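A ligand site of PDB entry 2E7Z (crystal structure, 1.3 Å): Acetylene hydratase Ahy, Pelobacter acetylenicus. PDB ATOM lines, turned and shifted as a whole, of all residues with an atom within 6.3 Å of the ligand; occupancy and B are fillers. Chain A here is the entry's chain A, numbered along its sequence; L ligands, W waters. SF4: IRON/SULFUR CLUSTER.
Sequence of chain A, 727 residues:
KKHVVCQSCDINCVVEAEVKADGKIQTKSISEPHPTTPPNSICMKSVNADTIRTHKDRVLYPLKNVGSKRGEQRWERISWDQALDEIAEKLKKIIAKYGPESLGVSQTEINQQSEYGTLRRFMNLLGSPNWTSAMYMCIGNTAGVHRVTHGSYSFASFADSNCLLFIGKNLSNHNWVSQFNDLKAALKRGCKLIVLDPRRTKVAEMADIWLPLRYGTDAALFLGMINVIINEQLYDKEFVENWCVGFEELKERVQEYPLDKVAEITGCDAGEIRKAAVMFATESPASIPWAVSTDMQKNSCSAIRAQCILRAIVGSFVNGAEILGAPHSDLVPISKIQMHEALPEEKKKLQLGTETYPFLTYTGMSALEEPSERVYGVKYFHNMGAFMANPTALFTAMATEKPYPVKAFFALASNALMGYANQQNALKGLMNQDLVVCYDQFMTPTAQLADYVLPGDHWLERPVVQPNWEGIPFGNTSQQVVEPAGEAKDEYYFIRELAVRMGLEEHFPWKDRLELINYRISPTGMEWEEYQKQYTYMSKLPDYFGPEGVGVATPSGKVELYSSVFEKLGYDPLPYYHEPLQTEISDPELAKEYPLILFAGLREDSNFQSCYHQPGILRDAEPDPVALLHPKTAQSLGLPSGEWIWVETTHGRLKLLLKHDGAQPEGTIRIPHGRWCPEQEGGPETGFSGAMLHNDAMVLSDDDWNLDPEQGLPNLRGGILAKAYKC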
ATOM      1  N   CYS A   6      28.797 -12.730  -0.809  1.00  0.00           N
ATOM      2  CA  CYS A   6      27.842 -13.657  -0.273  1.00  0.00           C
ATOM      3  C   CYS A   6      26.975 -14.163  -1.405  1.00  0.00           C
ATOM      4  O   CYS A   6      26.428 -13.352  -2.176  1.00  0.00           O
ATOM      5  CB  CYS A   6      27.005 -12.938   0.766  1.00  0.00           C
ATOM      6  SG  CYS A   6      25.683 -13.969   1.434  1.00  0.00           S
ATOM      7  N   GLN A   7      26.859 -15.484  -1.519  1.00  0.00           N
ATOM      8  CA  GLN A   7      25.986 -16.091  -2.543  1.00  0.00           C
ATOM      9  C   GLN A   7      24.858 -16.863  -1.863  1.00  0.00           C
ATOM     10  O   GLN A   7      24.317 -17.812  -2.436  1.00  0.00           O
ATOM     11  CB  GLN A   7      26.810 -16.962  -3.482  1.00  0.00           C
ATOM     12  CG  GLN A   7      27.815 -16.099  -4.296  1.00  0.00           C
ATOM     13  CD  GLN A   7      29.165 -16.772  -4.536  1.00  0.00           C
ATOM     14  OE1 GLN A   7      29.262 -17.773  -5.265  1.00  0.00           O
ATOM     15  NE2 GLN A   7      30.219 -16.183  -3.978  1.00  0.00           N
ATOM     16  N   SER A   8      24.496 -16.441  -0.661  1.00  0.00           N
ATOM     17  CA  SER A   8      23.326 -17.010  -0.004  1.00  0.00           C
ATOM     18  C   SER A   8      22.031 -16.458  -0.598  1.00  0.00           C
ATOM     19  O   SER A   8      20.972 -17.051  -0.430  1.00  0.00           O
ATOM     20  CB  SER A   8      23.374 -16.813   1.513  1.00  0.00           C
ATOM     21  OG  SER A   8      24.223 -17.768   2.135  1.00  0.00           O
ATOM     22  N   CYS A   9      22.128 -15.359  -1.349  1.00  0.00           N
ATOM     23  CA  CYS A   9      21.069 -14.966  -2.272  1.00  0.00           C
ATOM     24  C   CYS A   9      21.754 -14.172  -3.385  1.00  0.00           C
ATOM     25  O   CYS A   9      22.973 -13.970  -3.350  1.00  0.00           O
ATOM     26  CB  CYS A   9      19.896 -14.210  -1.607  1.00  0.00           C
ATOM     27  SG  CYS A   9      20.001 -12.403  -1.460  1.00  0.00           S
ATOM     28  N   ASP A  10      20.974 -13.729  -4.354  1.00  0.00           N
ATOM     29  CA  ASP A  10      21.571 -13.268  -5.596  1.00  0.00           C
ATOM     30  C   ASP A  10      21.951 -11.777  -5.683  1.00  0.00           C
ATOM     31  O   ASP A  10      22.525 -11.347  -6.678  1.00  0.00           O
ATOM     32  CB  ASP A  10      20.719 -13.678  -6.797  1.00  0.00           C
ATOM     33  CG  ASP A  10      19.292 -13.148  -6.747  1.00  0.00           C
ATOM     34  OD1 ASP A  10      18.802 -12.711  -5.679  1.00  0.00           O
ATOM     35  OD2 ASP A  10      18.647 -13.224  -7.829  1.00  0.00           O
ATOM     36  N   ILE A  11      21.660 -10.989  -4.641  1.00  0.00           N
ATOM     37  CA  ILE A  11      22.085  -9.592  -4.681  1.00  0.00           C
ATOM     38  C   ILE A  11      23.596  -9.474  -4.423  1.00  0.00           C
ATOM     39  O   ILE A  11      24.204  -8.494  -4.859  1.00  0.00           O
ATOM     40  CB  ILE A  11      21.267  -8.680  -3.734  1.00  0.00           C
ATOM     41  CG1 ILE A  11      21.364  -7.210  -4.154  1.00  0.00           C
ATOM     42  CG2 ILE A  11      21.691  -8.868  -2.296  1.00  0.00           C
ATOM     43  CD1 ILE A  11      20.963  -6.908  -5.599  1.00  0.00           C
ATOM     44  N   ASN A  12      24.176 -10.478  -3.756  1.00  0.00           N
ATOM     45  CA  ASN A  12      25.636 -10.621  -3.663  1.00  0.00           C
ATOM     46  C   ASN A  12      26.341  -9.475  -2.910  1.00  0.00           C
ATOM     47  O   ASN A  12      27.380  -8.951  -3.357  1.00  0.00           O
ATOM     48  CB  ASN A  12      26.245 -10.776  -5.069  1.00  0.00           C
ATOM     49  CG  ASN A  12      25.963 -12.136  -5.731  1.00  0.00           C
ATOM     50  OD1 ASN A  12      26.316 -12.291  -6.896  1.00  0.00           O
ATOM     51  ND2 ASN A  12      25.378 -13.111  -5.022  1.00  0.00           N
ATOM     52  N   CYS A  13      25.795  -9.126  -1.748  1.00  0.00           N
ATOM     53  CA  CYS A  13      26.513  -8.255  -0.807  1.00  0.00           C
ATOM     54  C   CYS A  13      27.916  -8.802  -0.592  1.00  0.00           C
ATOM     55  O   CYS A  13      28.109 -10.004  -0.473  1.00  0.00           O
ATOM     56  CB  CYS A  13      25.848  -8.308   0.565  1.00  0.00           C
ATOM     57  SG  CYS A  13      24.071  -7.936   0.571  1.00  0.00           S
ATOM     58  N   VAL A  15      30.715  -9.352   1.992  1.00  0.00           N
ATOM     59  CA  VAL A  15      30.804  -9.484   3.445  1.00  0.00           C
ATOM     60  C   VAL A  15      32.249  -9.794   3.826  1.00  0.00           C
ATOM     61  O   VAL A  15      33.118  -9.956   2.969  1.00  0.00           O
ATOM     62  CB  VAL A  15      29.821 -10.597   3.979  1.00  0.00           C
ATOM     63  CG1 VAL A  15      28.365 -10.278   3.624  1.00  0.00           C
ATOM     64  CG2 VAL A  15      30.178 -11.967   3.417  1.00  0.00           C
ATOM     65  N   SER A  41      25.500  -4.225   5.711  1.00  0.00           N
ATOM     66  CA  SER A  41      24.810  -5.069   4.738  1.00  0.00           C
ATOM     67  C   SER A  41      25.150  -6.550   4.922  1.00  0.00           C
ATOM     68  O   SER A  41      26.000  -7.107   4.224  1.00  0.00           O
ATOM     69  CB  SER A  41      25.079  -4.586   3.312  1.00  0.00           C
ATOM     70  OG  SER A  41      24.649  -3.239   3.093  1.00  0.00           O
ATOM     71  N   ILE A  42      24.498  -7.175   5.900  1.00  0.00           N
ATOM     72  CA  ILE A  42      24.495  -8.620   6.047  1.00  0.00           C
ATOM     73  C   ILE A  42      23.186  -9.047   6.678  1.00  0.00           C
ATOM     74  O   ILE A  42      22.633  -8.315   7.503  1.00  0.00           O
ATOM     75  CB  ILE A  42      25.714  -9.146   6.848  1.00  0.00           C
ATOM     76  CG1 ILE A  42      25.893 -10.642   6.581  1.00  0.00           C
ATOM     77  CG2 ILE A  42      25.554  -8.831   8.362  1.00  0.00           C
ATOM     78  CD1 ILE A  42      27.173 -11.250   7.097  1.00  0.00           C
ATOM     79  N   CYS A  43      22.675 -10.219   6.303  1.00  0.00           N
ATOM     80  CA  CYS A  43      21.393 -10.709   6.832  1.00  0.00           C
ATOM     81  C   CYS A  43      21.574 -12.061   7.506  1.00  0.00           C
ATOM     82  O   CYS A  43      22.661 -12.623   7.500  1.00  0.00           O
ATOM     83  CB  CYS A  43      20.348 -10.798   5.714  1.00  0.00           C
ATOM     84  SG  CYS A  43      20.620 -12.241   4.644  1.00  0.00           S
ATOM     85  N   MET A  44      20.501 -12.576   8.131  1.00  0.00           N
ATOM     86  CA  MET A  44      20.575 -13.833   8.846  1.00  0.00           C
ATOM     87  C   MET A  44      21.007 -14.999   7.947  1.00  0.00           C
ATOM     88  O   MET A  44      21.655 -15.904   8.417  1.00  0.00           O
ATOM     89  CB  MET A  44      19.249 -14.175   9.557  1.00  0.00           C
ATOM     90  CG  MET A  44      18.060 -14.245   8.601  1.00  0.00           C
ATOM     91  SD  MET A  44      16.557 -14.685   9.489  1.00  0.00           S
ATOM     92  CE  MET A  44      16.216 -13.230  10.467  1.00  0.00           C
ATOM     93  N   LYS A  45      20.659 -14.954   6.654  1.00  0.00           N
ATOM     94  CA  LYS A  45      21.027 -16.061   5.758  1.00  0.00           C
ATOM     95  C   LYS A  45      22.538 -16.147   5.625  1.00  0.00           C
ATOM     96  O   LYS A  45      23.099 -17.250   5.599  1.00  0.00           O
ATOM     97  CB  LYS A  45      20.364 -15.918   4.389  1.00  0.00           C
ATOM     98  CG  LYS A  45      18.830 -15.946   4.507  1.00  0.00           C
ATOM     99  CD  LYS A  45      18.110 -15.860   3.158  1.00  0.00           C
ATOM    100  CE  LYS A  45      18.364 -14.557   2.416  1.00  0.00           C
ATOM    101  NZ  LYS A  45      17.913 -13.360   3.187  1.00  0.00           N
ATOM    102  N   SER A  46      23.178 -14.981   5.551  1.00  0.00           N
ATOM    103  CA  SER A  46      24.630 -14.925   5.456  1.00  0.00           C
ATOM    104  C   SER A  46      25.331 -15.176   6.779  1.00  0.00           C
ATOM    105  O   SER A  46      26.308 -15.920   6.848  1.00  0.00           O
ATOM    106  CB  SER A  46      25.058 -13.582   4.904  1.00  0.00           C
ATOM    107  OG  SER A  46      26.420 -13.595   4.521  1.00  0.00           O
ATOM    108  N   VAL A  47      24.828 -14.530   7.839  1.00  0.00           N
ATOM    109  CA  VAL A  47      25.404 -14.720   9.178  1.00  0.00           C
ATOM    110  C   VAL A  47      25.479 -16.187   9.543  1.00  0.00           C
ATOM    111  O   VAL A  47      26.447 -16.650  10.155  1.00  0.00           O
ATOM    112  CB  VAL A  47      24.575 -13.980  10.246  1.00  0.00           C
ATOM    113  CG1 VAL A  47      24.976 -14.436  11.669  1.00  0.00           C
ATOM    114  CG2 VAL A  47      24.756 -12.490  10.074  1.00  0.00           C
ATOM    115  N   ASN A 173      16.067  -5.914   6.598  1.00  0.00           N
ATOM    116  CA  ASN A 173      17.340  -6.402   7.088  1.00  0.00           C
ATOM    117  C   ASN A 173      17.639  -7.845   6.691  1.00  0.00           C
ATOM    118  O   ASN A 173      18.756  -8.300   6.871  1.00  0.00           O
ATOM    119  CB  ASN A 173      17.457  -6.184   8.593  1.00  0.00           C
ATOM    120  CG  ASN A 173      17.924  -4.791   8.930  1.00  0.00           C
ATOM    121  OD1 ASN A 173      18.631  -4.147   8.146  1.00  0.00           O
ATOM    122  ND2 ASN A 173      17.530  -4.306  10.106  1.00  0.00           N
ATOM    123  N   HIS A 174      16.641  -8.547   6.150  1.00  0.00           N
ATOM    124  CA  HIS A 174      16.897  -9.924   5.694  1.00  0.00           C
ATOM    125  C   HIS A 174      16.334 -10.261   4.317  1.00  0.00           C
ATOM    126  O   HIS A 174      16.194 -11.433   3.951  1.00  0.00           O
ATOM    127  CB  HIS A 174      16.450 -10.964   6.734  1.00  0.00           C
ATOM    128  CG  HIS A 174      16.977 -10.702   8.102  1.00  0.00           C
ATOM    129  ND1 HIS A 174      18.227 -11.115   8.516  1.00  0.00           N
ATOM    130  CD2 HIS A 174      16.425 -10.058   9.160  1.00  0.00           C
ATOM    131  CE1 HIS A 174      18.429 -10.741   9.770  1.00  0.00           C
ATOM    132  NE2 HIS A 174      17.348 -10.090  10.184  1.00  0.00           N
ATOM    133  N   ASN A 175      16.004  -9.221   3.555  1.00  0.00           N
ATOM    134  CA  ASN A 175      15.670  -9.362   2.139  1.00  0.00           C
ATOM    135  C   ASN A 175      16.493  -8.338   1.406  1.00  0.00           C
ATOM    136  O   ASN A 175      16.205  -7.126   1.477  1.00  0.00           O
ATOM    137  CB  ASN A 175      14.169  -9.163   1.907  1.00  0.00           C
ATOM    138  CG  ASN A 175      13.757  -9.317   0.432  1.00  0.00           C
ATOM    139  OD1 ASN A 175      14.590  -9.198  -0.478  1.00  0.00           O
ATOM    140  ND2 ASN A 175      12.486  -9.584   0.208  1.00  0.00           N
ATOM    141  N   TRP A 176      17.548  -8.802   0.724  1.00  0.00           N
ATOM    142  CA  TRP A 176      18.410  -7.922  -0.049  1.00  0.00           C
ATOM    143  C   TRP A 176      18.850  -6.736   0.821  1.00  0.00           C
ATOM    144  O   TRP A 176      18.614  -5.573   0.479  1.00  0.00           O
ATOM    145  CB  TRP A 176      17.696  -7.476  -1.321  1.00  0.00           C
ATOM    146  CG  TRP A 176      17.829  -8.430  -2.487  1.00  0.00           C
ATOM    147  CD1 TRP A 176      18.103  -9.780  -2.443  1.00  0.00           C
ATOM    148  CD2 TRP A 176      17.656  -8.110  -3.860  1.00  0.00           C
ATOM    149  NE1 TRP A 176      18.151 -10.298  -3.727  1.00  0.00           N
ATOM    150  CE2 TRP A 176      17.865  -9.289  -4.612  1.00  0.00           C
ATOM    151  CE3 TRP A 176      17.365  -6.917  -4.537  1.00  0.00           C
ATOM    152  CZ2 TRP A 176      17.785  -9.319  -6.015  1.00  0.00           C
ATOM    153  CZ3 TRP A 176      17.284  -6.943  -5.926  1.00  0.00           C
ATOM    154  CH2 TRP A 176      17.493  -8.134  -6.650  1.00  0.00           C
ATOM    155  N   VAL A 177      19.478  -7.049   1.944  1.00  0.00           N
ATOM    156  CA  VAL A 177      19.836  -6.034   2.948  1.00  0.00           C
ATOM    157  C   VAL A 177      20.728  -4.902   2.380  1.00  0.00           C
ATOM    158  O   VAL A 177      20.548  -3.733   2.725  1.00  0.00           O
ATOM    159  CB  VAL A 177      20.433  -6.694   4.218  1.00  0.00           C
ATOM    160  CG1 VAL A 177      21.689  -7.459   3.896  1.00  0.00           C
ATOM    161  CG2 VAL A 177      20.676  -5.654   5.320  1.00  0.00           C
ATOM    162  N   SER A 178      21.669  -5.250   1.510  1.00  0.00           N
ATOM    163  CA  SER A 178      22.478  -4.199   0.864  1.00  0.00           C
ATOM    164  C   SER A 178      21.608  -3.180   0.139  1.00  0.00           C
ATOM    165  O   SER A 178      21.820  -1.977   0.290  1.00  0.00           O
ATOM    166  CB  SER A 178      23.527  -4.805  -0.073  1.00  0.00           C
ATOM    167  OG  SER A 178      22.930  -5.690  -1.010  1.00  0.00           O
ATOM    168  N   TRP A 459      29.766 -21.163  -1.351  1.00  0.00           N
ATOM    169  CA  TRP A 459      30.369 -19.846  -1.557  1.00  0.00           C
ATOM    170  C   TRP A 459      31.499 -19.473  -0.580  1.00  0.00           C
ATOM    171  O   TRP A 459      32.280 -18.577  -0.868  1.00  0.00           O
ATOM    172  CB  TRP A 459      29.290 -18.746  -1.637  1.00  0.00           C
ATOM    173  CG  TRP A 459      28.505 -18.446  -0.397  1.00  0.00           C
ATOM    174  CD1 TRP A 459      27.257 -18.935  -0.096  1.00  0.00           C
ATOM    175  CD2 TRP A 459      28.826 -17.496   0.623  1.00  0.00           C
ATOM    176  NE1 TRP A 459      26.816 -18.365   1.104  1.00  0.00           N
ATOM    177  CE2 TRP A 459      27.764 -17.485   1.548  1.00  0.00           C
ATOM    178  CE3 TRP A 459      29.931 -16.655   0.854  1.00  0.00           C
ATOM    179  CZ2 TRP A 459      27.770 -16.646   2.675  1.00  0.00           C
ATOM    180  CZ3 TRP A 459      29.918 -15.828   1.954  1.00  0.00           C
ATOM    181  CH2 TRP A 459      28.848 -15.837   2.848  1.00  0.00           C
ATOM    182  N   TYR A 612      17.807 -23.603   2.394  1.00  0.00           N
ATOM    183  CA  TYR A 612      18.026 -23.399   3.848  1.00  0.00           C
ATOM    184  C   TYR A 612      16.857 -23.885   4.693  1.00  0.00           C
ATOM    185  O   TYR A 612      16.707 -23.456   5.864  1.00  0.00           O
ATOM    186  CB  TYR A 612      18.449 -21.944   4.235  1.00  0.00           C
ATOM    187  CG  TYR A 612      19.331 -21.308   3.217  1.00  0.00           C
ATOM    188  CD1 TYR A 612      20.332 -22.045   2.583  1.00  0.00           C
ATOM    189  CD2 TYR A 612      19.115 -19.975   2.839  1.00  0.00           C
ATOM    190  CE1 TYR A 612      21.117 -21.450   1.570  1.00  0.00           C
ATOM    191  CE2 TYR A 612      19.880 -19.384   1.857  1.00  0.00           C
ATOM    192  CZ  TYR A 612      20.871 -20.128   1.209  1.00  0.00           C
ATOM    193  OH  TYR A 612      21.597 -19.546   0.191  1.00  0.00           O
HETATM  194 FE1  SF4 L   1      21.796 -11.532   2.787  1.00  0.00          FE
HETATM  195 FE2  SF4 L   1      23.871 -12.546   1.420  1.00  0.00          FE
HETATM  196 FE3  SF4 L   1      23.127  -9.976   1.037  1.00  0.00          FE
HETATM  197 FE4  SF4 L   1      21.596 -11.968   0.115  1.00  0.00          FE
HETATM  198  S1  SF4 L   1      23.676 -11.501  -0.613  1.00  0.00           S
HETATM  199  S2  SF4 L   1      20.854 -10.080   1.236  1.00  0.00           S
HETATM  200  S3  SF4 L   1      21.895 -13.594   1.737  1.00  0.00           S
HETATM  201  S4  SF4 L   1      23.954 -10.861   3.003  1.00  0.00           S
HETATM  202  O   HOH W   1      17.788 -11.545   0.764  1.00  0.00           O
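Water W1 lies within hydrogen-bond range of N of Trp 176 (2.8 Å), NZ of Lys 45 (3.0 Å) and S2 of the ligand (3.4 Å).
The backbone carbonyl oxygen (O) of Cys 13 is in hydrogen-bond range of the backbone NH (N) of Cys 6, at 2.8 Å. OG of Ser 46 lies close to SG of Cys 6 (3.2 Å). The side-chain sulfur (SG) of Cys 6 lies close to the backbone NH (N) of Ser 8 (3.5 Å). The side-chain amino group (NZ) of Lys 45 lies close to the side-chain sulfur (SG) of Cys 43. The indole nitrogen (NE1) of Trp 176 sits at hydrogen-bond distance from the side-chain carboxylate (OD1) of Asp 10 (3.2 Å). OG of Ser 8 is in hydrogen-bond range of NE1 of Trp 459 (2.9 Å). The backbone carbonyl oxygen (O) of Ser 8 lies within hydrogen-bond range of the side-chain hydroxyl (OH) of Tyr 612, 2.6 Å away. The backbone carbonyl oxygen of His 174 is in hydrogen-bond range of the side-chain amino group of Lys 45 (2.7 Å).
CB of Ser 8 touches S3 of the ligand, at 3.5 Å. Ile 11 touches the ligand (CG2 to S1, 3.7 Å). Ile 42 touches the ligand. Lys 45 touches the ligand (CE to S3, 3.7 Å). Ser 46 touches the ligand. Hydrophobic or aromatic side chains within 4 Å of the ligand: Ile 11 and Val 177. 12 residues have an atom within 4 Å of the ligand: Cys 6, Ser 8, Cys 9, Ile 11, Asn 12, Cys 13, Ile 42, Cys 43, Lys 45, Ser 46, Trp 176 and Val 177. The nearest printed residue that does not touch the ligand is Ser 41 (4.4 Å).
N of Cys 9 sits close to S3 of the ligand, at 3.6 Å. The side-chain sulfur (SG) of Cys 9 is bound to an iron atom (FE4) of the ligand (2.3 Å). N of Cys 13 lies close to S1 of the ligand. The side-chain sulfur of Cys 13 binds an iron atom (FE3) of the ligand (2.3 Å). An iron atom (FE2) of the ligand is bound by the side-chain sulfur (SG) of Cys 6 (2.3 Å). A sulfur (S4) of the ligand sits close to the backbone NH (N) of Cys 43 (3.6 Å). FE1 of the ligand is bound by SG of Cys 43 (2.3 Å). The backbone NH (N) of Asn 12 lies close to a sulfur (S1) of the ligand. N of Val 177 lies close to S2 of the ligand. N of Trp 176 lies close to S2 of the ligand, at 3.6 Å.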
